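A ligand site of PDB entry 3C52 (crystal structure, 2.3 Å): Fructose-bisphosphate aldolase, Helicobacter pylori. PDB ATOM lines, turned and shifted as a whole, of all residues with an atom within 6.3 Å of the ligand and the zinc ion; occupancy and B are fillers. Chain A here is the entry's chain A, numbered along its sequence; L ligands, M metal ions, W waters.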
ATOM      1  N   ALA A  21      29.805 -22.427 -29.081  1.00  0.00           N
ATOM      2  CA  ALA A  21      29.754 -21.630 -30.287  1.00  0.00           C
ATOM      3  C   ALA A  21      29.468 -20.223 -29.787  1.00  0.00           C
ATOM      4  O   ALA A  21      28.391 -19.947 -29.246  1.00  0.00           O
ATOM      5  CB  ALA A  21      28.663 -22.088 -31.200  1.00  0.00           C
ATOM      6  N   ASN A  23      29.171 -16.148 -30.266  1.00  0.00           N
ATOM      7  CA  ASN A  23      28.883 -15.070 -31.201  1.00  0.00           C
ATOM      8  C   ASN A  23      29.735 -13.855 -30.952  1.00  0.00           C
ATOM      9  O   ASN A  23      30.100 -13.577 -29.810  1.00  0.00           O
ATOM     10  CB  ASN A  23      27.424 -14.664 -31.102  1.00  0.00           C
ATOM     11  CG  ASN A  23      26.500 -15.667 -31.701  1.00  0.00           C
ATOM     12  OD1 ASN A  23      26.296 -16.743 -31.148  1.00  0.00           O
ATOM     13  ND2 ASN A  23      25.919 -15.322 -32.847  1.00  0.00           N
ATOM     14  N   GLN A  47      31.001 -17.720 -34.166  1.00  0.00           N
ATOM     15  CA  GLN A  47      29.867 -17.458 -35.040  1.00  0.00           C
ATOM     16  C   GLN A  47      29.296 -16.031 -35.068  1.00  0.00           C
ATOM     17  O   GLN A  47      29.271 -15.312 -34.059  1.00  0.00           O
ATOM     18  CB  GLN A  47      28.754 -18.483 -34.814  1.00  0.00           C
ATOM     19  CG  GLN A  47      28.268 -18.612 -33.407  1.00  0.00           C
ATOM     20  CD  GLN A  47      27.143 -19.617 -33.308  1.00  0.00           C
ATOM     21  OE1 GLN A  47      27.162 -20.652 -33.979  1.00  0.00           O
ATOM     22  NE2 GLN A  47      26.159 -19.332 -32.468  1.00  0.00           N
ATOM     23  N   ASP A  82      25.491 -18.062 -38.356  1.00  0.00           N
ATOM     24  CA  ASP A  82      24.499 -18.418 -37.380  1.00  0.00           C
ATOM     25  C   ASP A  82      23.149 -17.964 -37.895  1.00  0.00           C
ATOM     26  O   ASP A  82      23.005 -16.813 -38.290  1.00  0.00           O
ATOM     27  CB  ASP A  82      24.834 -17.726 -36.067  1.00  0.00           C
ATOM     28  CG  ASP A  82      23.942 -18.155 -34.929  1.00  0.00           C
ATOM     29  OD1 ASP A  82      23.335 -19.239 -35.025  1.00  0.00           O
ATOM     30  OD2 ASP A  82      23.836 -17.401 -33.942  1.00  0.00           O
ATOM     31  N   HIS A  83      22.197 -18.889 -37.916  1.00  0.00           N
ATOM     32  CA  HIS A  83      20.862 -18.647 -38.481  1.00  0.00           C
ATOM     33  C   HIS A  83      20.871 -17.985 -39.865  1.00  0.00           C
ATOM     34  O   HIS A  83      20.376 -16.880 -40.028  1.00  0.00           O
ATOM     35  CB  HIS A  83      19.992 -17.833 -37.526  1.00  0.00           C
ATOM     36  CG  HIS A  83      19.691 -18.564 -36.255  1.00  0.00           C
ATOM     37  ND1 HIS A  83      18.623 -19.412 -36.132  1.00  0.00           N
ATOM     38  CD2 HIS A  83      20.318 -18.581 -35.052  1.00  0.00           C
ATOM     39  CE1 HIS A  83      18.590 -19.921 -34.913  1.00  0.00           C
ATOM     40  NE2 HIS A  83      19.621 -19.434 -34.244  1.00  0.00           N
ATOM     41  N   MET A 102      24.866 -22.178 -41.061  1.00  0.00           N
ATOM     42  CA  MET A 102      23.607 -22.791 -40.651  1.00  0.00           C
ATOM     43  C   MET A 102      22.513 -22.260 -41.562  1.00  0.00           C
ATOM     44  O   MET A 102      22.438 -21.045 -41.810  1.00  0.00           O
ATOM     45  CB  MET A 102      23.251 -22.505 -39.204  1.00  0.00           C
ATOM     46  CG  MET A 102      21.864 -22.987 -38.860  1.00  0.00           C
ATOM     47  SD  MET A 102      21.186 -22.160 -37.419  1.00  0.00           S
ATOM     48  CE  MET A 102      19.833 -23.265 -37.011  1.00  0.00           C
ATOM     49  N   GLU A 134      18.106 -26.956 -38.795  1.00  0.00           N
ATOM     50  CA  GLU A 134      17.289 -27.103 -37.595  1.00  0.00           C
ATOM     51  C   GLU A 134      16.004 -27.856 -37.861  1.00  0.00           C
ATOM     52  O   GLU A 134      15.425 -27.775 -38.944  1.00  0.00           O
ATOM     53  CB  GLU A 134      16.975 -25.735 -36.989  1.00  0.00           C
ATOM     54  CG  GLU A 134      16.081 -25.799 -35.754  1.00  0.00           C
ATOM     55  CD  GLU A 134      15.892 -24.461 -35.070  1.00  0.00           C
ATOM     56  OE1 GLU A 134      16.655 -23.526 -35.385  1.00  0.00           O
ATOM     57  OE2 GLU A 134      14.979 -24.342 -34.226  1.00  0.00           O
ATOM     58  N   LEU A 138      12.262 -23.124 -31.751  1.00  0.00           N
ATOM     59  CA  LEU A 138      12.802 -22.761 -30.440  1.00  0.00           C
ATOM     60  C   LEU A 138      11.830 -22.058 -29.496  1.00  0.00           C
ATOM     61  O   LEU A 138      11.860 -20.842 -29.339  1.00  0.00           O
ATOM     62  CB  LEU A 138      14.086 -21.938 -30.611  1.00  0.00           C
ATOM     63  CG  LEU A 138      15.277 -22.724 -31.146  1.00  0.00           C
ATOM     64  CD1 LEU A 138      16.357 -21.803 -31.685  1.00  0.00           C
ATOM     65  CD2 LEU A 138      15.832 -23.650 -30.081  1.00  0.00           C
ATOM     66  N   SER A 179      15.108 -21.740 -25.939  1.00  0.00           N
ATOM     67  CA  SER A 179      14.814 -20.607 -26.815  1.00  0.00           C
ATOM     68  C   SER A 179      15.879 -19.553 -26.597  1.00  0.00           C
ATOM     69  O   SER A 179      16.527 -19.549 -25.537  1.00  0.00           O
ATOM     70  CB  SER A 179      13.423 -20.037 -26.530  1.00  0.00           C
ATOM     71  OG  SER A 179      13.283 -19.689 -25.164  1.00  0.00           O
ATOM     72  N   HIS A 180      16.057 -18.675 -27.580  1.00  0.00           N
ATOM     73  CA  HIS A 180      17.068 -17.619 -27.494  1.00  0.00           C
ATOM     74  C   HIS A 180      16.714 -16.553 -26.448  1.00  0.00           C
ATOM     75  O   HIS A 180      15.541 -16.408 -26.090  1.00  0.00           O
ATOM     76  CB  HIS A 180      17.262 -16.971 -28.875  1.00  0.00           C
ATOM     77  CG  HIS A 180      17.658 -17.932 -29.949  1.00  0.00           C
ATOM     78  ND1 HIS A 180      17.206 -17.836 -31.244  1.00  0.00           N
ATOM     79  CD2 HIS A 180      18.447 -19.034 -29.902  1.00  0.00           C
ATOM     80  CE1 HIS A 180      17.710 -18.822 -31.964  1.00  0.00           C
ATOM     81  NE2 HIS A 180      18.466 -19.565 -31.174  1.00  0.00           N
ATOM     82  N   GLY A 181      17.722 -15.827 -25.975  1.00  0.00           N
ATOM     83  CA  GLY A 181      17.483 -14.736 -25.048  1.00  0.00           C
ATOM     84  C   GLY A 181      17.558 -15.060 -23.560  1.00  0.00           C
ATOM     85  O   GLY A 181      17.725 -16.216 -23.160  1.00  0.00           O
ATOM     86  N   ALA A 182      17.433 -14.018 -22.741  1.00  0.00           N
ATOM     87  CA  ALA A 182      17.633 -14.123 -21.296  1.00  0.00           C
ATOM     88  C   ALA A 182      16.463 -14.749 -20.552  1.00  0.00           C
ATOM     89  O   ALA A 182      16.562 -15.045 -19.355  1.00  0.00           O
ATOM     90  CB  ALA A 182      17.964 -12.752 -20.721  1.00  0.00           C
ATOM     91  N   LYS A 184      14.332 -17.869 -20.940  1.00  0.00           N
ATOM     92  CA  LYS A 184      14.095 -19.137 -21.624  1.00  0.00           C
ATOM     93  C   LYS A 184      12.977 -19.991 -20.989  1.00  0.00           C
ATOM     94  O   LYS A 184      12.149 -20.567 -21.708  1.00  0.00           O
ATOM     95  CB  LYS A 184      15.383 -19.965 -21.684  1.00  0.00           C
ATOM     96  CG  LYS A 184      16.509 -19.244 -22.416  1.00  0.00           C
ATOM     97  CD  LYS A 184      17.785 -20.048 -22.403  1.00  0.00           C
ATOM     98  CE  LYS A 184      18.956 -19.170 -22.842  1.00  0.00           C
ATOM     99  NZ  LYS A 184      18.653 -18.510 -24.136  1.00  0.00           N
ATOM    100  N   LEU A 209      22.959 -27.280 -29.760  1.00  0.00           N
ATOM    101  CA  LEU A 209      21.976 -26.745 -28.827  1.00  0.00           C
ATOM    102  C   LEU A 209      21.917 -25.228 -28.947  1.00  0.00           C
ATOM    103  O   LEU A 209      22.898 -24.521 -28.629  1.00  0.00           O
ATOM    104  CB  LEU A 209      22.266 -27.142 -27.390  1.00  0.00           C
ATOM    105  CG  LEU A 209      21.211 -26.651 -26.391  1.00  0.00           C
ATOM    106  CD1 LEU A 209      19.915 -27.456 -26.530  1.00  0.00           C
ATOM    107  CD2 LEU A 209      21.712 -26.732 -24.963  1.00  0.00           C
ATOM    108  N   HIS A 210      20.779 -24.720 -29.423  1.00  0.00           N
ATOM    109  CA  HIS A 210      20.557 -23.293 -29.515  1.00  0.00           C
ATOM    110  C   HIS A 210      19.947 -22.794 -28.237  1.00  0.00           C
ATOM    111  O   HIS A 210      19.400 -23.574 -27.456  1.00  0.00           O
ATOM    112  CB  HIS A 210      19.627 -22.975 -30.675  1.00  0.00           C
ATOM    113  CG  HIS A 210      20.310 -22.980 -32.006  1.00  0.00           C
ATOM    114  ND1 HIS A 210      20.481 -21.831 -32.753  1.00  0.00           N
ATOM    115  CD2 HIS A 210      20.902 -23.969 -32.703  1.00  0.00           C
ATOM    116  CE1 HIS A 210      21.124 -22.128 -33.864  1.00  0.00           C
ATOM    117  NE2 HIS A 210      21.397 -23.419 -33.849  1.00  0.00           N
ATOM    118  N   GLY A 211      20.028 -21.479 -28.045  1.00  0.00           N
ATOM    119  CA  GLY A 211      19.467 -20.843 -26.872  1.00  0.00           C
ATOM    120  C   GLY A 211      20.050 -21.424 -25.600  1.00  0.00           C
ATOM    121  O   GLY A 211      19.341 -21.617 -24.607  1.00  0.00           O
ATOM    122  N   ALA A 212      21.360 -21.669 -25.635  1.00  0.00           N
ATOM    123  CA  ALA A 212      22.059 -22.390 -24.566  1.00  0.00           C
ATOM    124  C   ALA A 212      22.770 -21.533 -23.518  1.00  0.00           C
ATOM    125  O   ALA A 212      23.572 -22.048 -22.753  1.00  0.00           O
ATOM    126  CB  ALA A 212      23.038 -23.380 -25.165  1.00  0.00           C
ATOM    127  N   SER A 213      22.489 -20.236 -23.475  1.00  0.00           N
ATOM    128  CA  SER A 213      23.094 -19.426 -22.423  1.00  0.00           C
ATOM    129  C   SER A 213      22.573 -19.892 -21.074  1.00  0.00           C
ATOM    130  O   SER A 213      21.471 -20.439 -20.976  1.00  0.00           O
ATOM    131  CB  SER A 213      22.850 -17.934 -22.618  1.00  0.00           C
ATOM    132  OG  SER A 213      23.799 -17.395 -23.522  1.00  0.00           O
ATOM    133  N   ALA A 214      23.388 -19.675 -20.039  1.00  0.00           N
ATOM    134  CA  ALA A 214      23.140 -20.234 -18.730  1.00  0.00           C
ATOM    135  C   ALA A 214      22.629 -19.152 -17.788  1.00  0.00           C
ATOM    136  O   ALA A 214      21.826 -19.425 -16.884  1.00  0.00           O
ATOM    137  CB  ALA A 214      24.412 -20.841 -18.187  1.00  0.00           C
ATOM    138  N   ASN A 253      25.419 -23.209 -28.561  1.00  0.00           N
ATOM    139  CA  ASN A 253      25.380 -21.799 -28.954  1.00  0.00           C
ATOM    140  C   ASN A 253      25.228 -20.870 -27.761  1.00  0.00           C
ATOM    141  O   ASN A 253      24.288 -21.005 -26.973  1.00  0.00           O
ATOM    142  CB  ASN A 253      24.240 -21.546 -29.935  1.00  0.00           C
ATOM    143  CG  ASN A 253      24.443 -22.265 -31.245  1.00  0.00           C
ATOM    144  OD1 ASN A 253      25.373 -23.039 -31.409  1.00  0.00           O
ATOM    145  ND2 ASN A 253      23.565 -22.009 -32.191  1.00  0.00           N
ATOM    146  N   THR A 254      26.152 -19.923 -27.638  1.00  0.00           N
ATOM    147  CA  THR A 254      26.227 -19.064 -26.475  1.00  0.00           C
ATOM    148  C   THR A 254      26.424 -17.619 -26.910  1.00  0.00           C
ATOM    149  O   THR A 254      27.406 -17.301 -27.568  1.00  0.00           O
ATOM    150  CB  THR A 254      27.432 -19.479 -25.603  1.00  0.00           C
ATOM    151  OG1 THR A 254      27.524 -20.909 -25.560  1.00  0.00           O
ATOM    152  CG2 THR A 254      27.300 -18.937 -24.189  1.00  0.00           C
ATOM    153  N   ASP A 255      25.509 -16.741 -26.552  1.00  0.00           N
ATOM    154  CA  ASP A 255      25.582 -15.353 -27.002  1.00  0.00           C
ATOM    155  C   ASP A 255      25.142 -14.385 -25.897  1.00  0.00           C
ATOM    156  O   ASP A 255      25.914 -13.545 -25.449  1.00  0.00           O
ATOM    157  CB  ASP A 255      24.748 -15.158 -28.257  1.00  0.00           C
ATOM    158  CG  ASP A 255      24.839 -13.760 -28.794  1.00  0.00           C
ATOM    159  OD1 ASP A 255      25.666 -12.973 -28.280  1.00  0.00           O
ATOM    160  OD2 ASP A 255      24.079 -13.453 -29.738  1.00  0.00           O
ATOM    161  N   THR A 256      23.892 -14.517 -25.458  1.00  0.00           N
ATOM    162  CA  THR A 256      23.354 -13.675 -24.394  1.00  0.00           C
ATOM    163  C   THR A 256      24.292 -13.537 -23.191  1.00  0.00           C
ATOM    164  O   THR A 256      24.431 -12.446 -22.613  1.00  0.00           O
ATOM    165  CB  THR A 256      22.002 -14.256 -23.906  1.00  0.00           C
ATOM    166  OG1 THR A 256      21.033 -14.145 -24.958  1.00  0.00           O
ATOM    167  CG2 THR A 256      21.518 -13.502 -22.678  1.00  0.00           C
ATOM    168  N   ASP A 257      24.918 -14.625 -22.787  1.00  0.00           N
ATOM    169  CA  ASP A 257      25.805 -14.610 -21.620  1.00  0.00           C
ATOM    170  C   ASP A 257      26.976 -13.641 -21.816  1.00  0.00           C
ATOM    171  O   ASP A 257      27.328 -12.905 -20.900  1.00  0.00           O
ATOM    172  CB  ASP A 257      26.313 -16.011 -21.304  1.00  0.00           C
ATOM    173  CG  ASP A 257      25.352 -16.791 -20.400  1.00  0.00           C
ATOM    174  OD1 ASP A 257      24.328 -16.206 -19.973  1.00  0.00           O
ATOM    175  OD2 ASP A 257      25.627 -17.979 -20.120  1.00  0.00           O
ATOM    176  N   ARG A 259      27.155 -10.993 -23.941  1.00  0.00           N
ATOM    177  CA  ARG A 259      26.642  -9.624 -24.032  1.00  0.00           C
ATOM    178  C   ARG A 259      26.312  -9.021 -22.668  1.00  0.00           C
ATOM    179  O   ARG A 259      26.643  -7.866 -22.390  1.00  0.00           O
ATOM    180  CB  ARG A 259      25.418  -9.582 -24.957  1.00  0.00           C
ATOM    181  CG  ARG A 259      25.745  -9.896 -26.410  1.00  0.00           C
ATOM    182  CD  ARG A 259      24.640 -10.665 -27.127  1.00  0.00           C
ATOM    183  NE  ARG A 259      23.424  -9.896 -27.385  1.00  0.00           N
ATOM    184  CZ  ARG A 259      22.515 -10.252 -28.292  1.00  0.00           C
ATOM    185  NH1 ARG A 259      22.674 -11.343 -29.008  1.00  0.00           N
ATOM    186  NH2 ARG A 259      21.429  -9.505 -28.487  1.00  0.00           N
HETATM  187  C1  LIG L   1      22.052 -19.071 -29.891  1.00  0.00           C
HETATM  188  C2  LIG L   1      22.351 -18.192 -28.677  1.00  0.00           C
HETATM  189  N1  LIG L   1      22.844 -18.931 -31.103  1.00  0.00           N
HETATM  190  O1  LIG L   1      22.219 -18.942 -32.356  1.00  0.00           O
HETATM  191  O2  LIG L   1      21.171 -19.873 -29.849  1.00  0.00           O
HETATM  192  O3  LIG L   1      21.421 -18.469 -27.659  1.00  0.00           O
HETATM  193  O4  LIG L   1      20.972 -18.547 -24.991  1.00  0.00           O
HETATM  194  O5  LIG L   1      23.000 -17.067 -25.980  1.00  0.00           O
HETATM  195  O6  LIG L   1      20.558 -16.444 -26.361  1.00  0.00           O
HETATM  196  P1  LIG L   1      21.460 -17.592 -26.252  1.00  0.00           P
HETATM  197 ZN    ZN M   1      20.178 -19.738 -32.366  1.00  0.00          ZN
HETATM  198  O   HOH W   1      20.555 -15.248 -28.663  1.00  0.00           O
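A ring nitrogen (NE2) of His 210 sits close to the side-chain amide nitrogen (ND2) of Asn 253, at 3.1 Å.
A ring nitrogen (NE2) of His 210 lies close to the side-chain sulfur (SD) of Met 102 (3.8 Å).
OG of Ser 213 is in hydrogen-bond range of N of Asp 257, 3.1 Å away.
NE2 of Gln 47 lies within hydrogen-bond range of OD2 of Asp 82, 3.4 Å away.
O of Asn 253 sits close to N of Ala 212 (3.3 Å).
The backbone NH (N) of Asn 253 lies within hydrogen-bond range of the backbone carbonyl oxygen (O) of Leu 209, 2.8 Å away.
O of Thr 254 is in hydrogen-bond range of N of Asn 23.
The backbone NH (N) of Thr 254 is in hydrogen-bond range of the backbone carbonyl oxygen (O) of Ala 21.
The zinc ion is bound by NE2 of His 83, NE2 of His 180, ND1 of His 210 and O1 of the ligand.
Slightly farther from the zinc ion lies an oxygen (O2) of the ligand (2.7 Å).
Gln 47 touches the ligand.
Thr 254 touches the ligand (C to O5, 3.6 Å).
14 residues have an atom within 4 Å of the ligand: Gln 47, Asp 82, His 83, His 180, Gly 181, Lys 184, His 210, Gly 211, Ala 212, Ser 213, Asn 253, Thr 254, Asp 255 and Thr 256.
O4 of the ligand is in salt-bridge range of NZ of Lys 184 (2.5 Å).
The backbone NH (N) of Asp 255 is in hydrogen-bond range of an oxygen (O5) of the ligand.
O4 of the ligand is in hydrogen-bond range of N of Ser 213 (2.7 Å).
The side-chain hydroxyl of Ser 213 is in hydrogen-bond range of an oxygen (O5) of the ligand (2.6 Å).
O2 of the ligand is in hydrogen-bond range of N of Gly 211, 2.7 Å away.
The backbone NH (N) of Thr 256 sits at hydrogen-bond distance from an oxygen (O5) of the ligand.
An oxygen (O6) of the ligand sits at hydrogen-bond distance from the side-chain hydroxyl (OG1) of Thr 256, 2.7 Å away.
OD2 of Asp 82 is in hydrogen-bond range of N1 of the ligand.
An oxygen (O6) of the ligand is in hydrogen-bond range of the backbone NH (N) of Gly 181, 2.9 Å away.
ND2 of Asn 253 lies close to N1 of the ligand, 3.3 Å away.
The backbone NH (N) of Ala 212 lies within hydrogen-bond range of an oxygen (O4) of the ligand.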
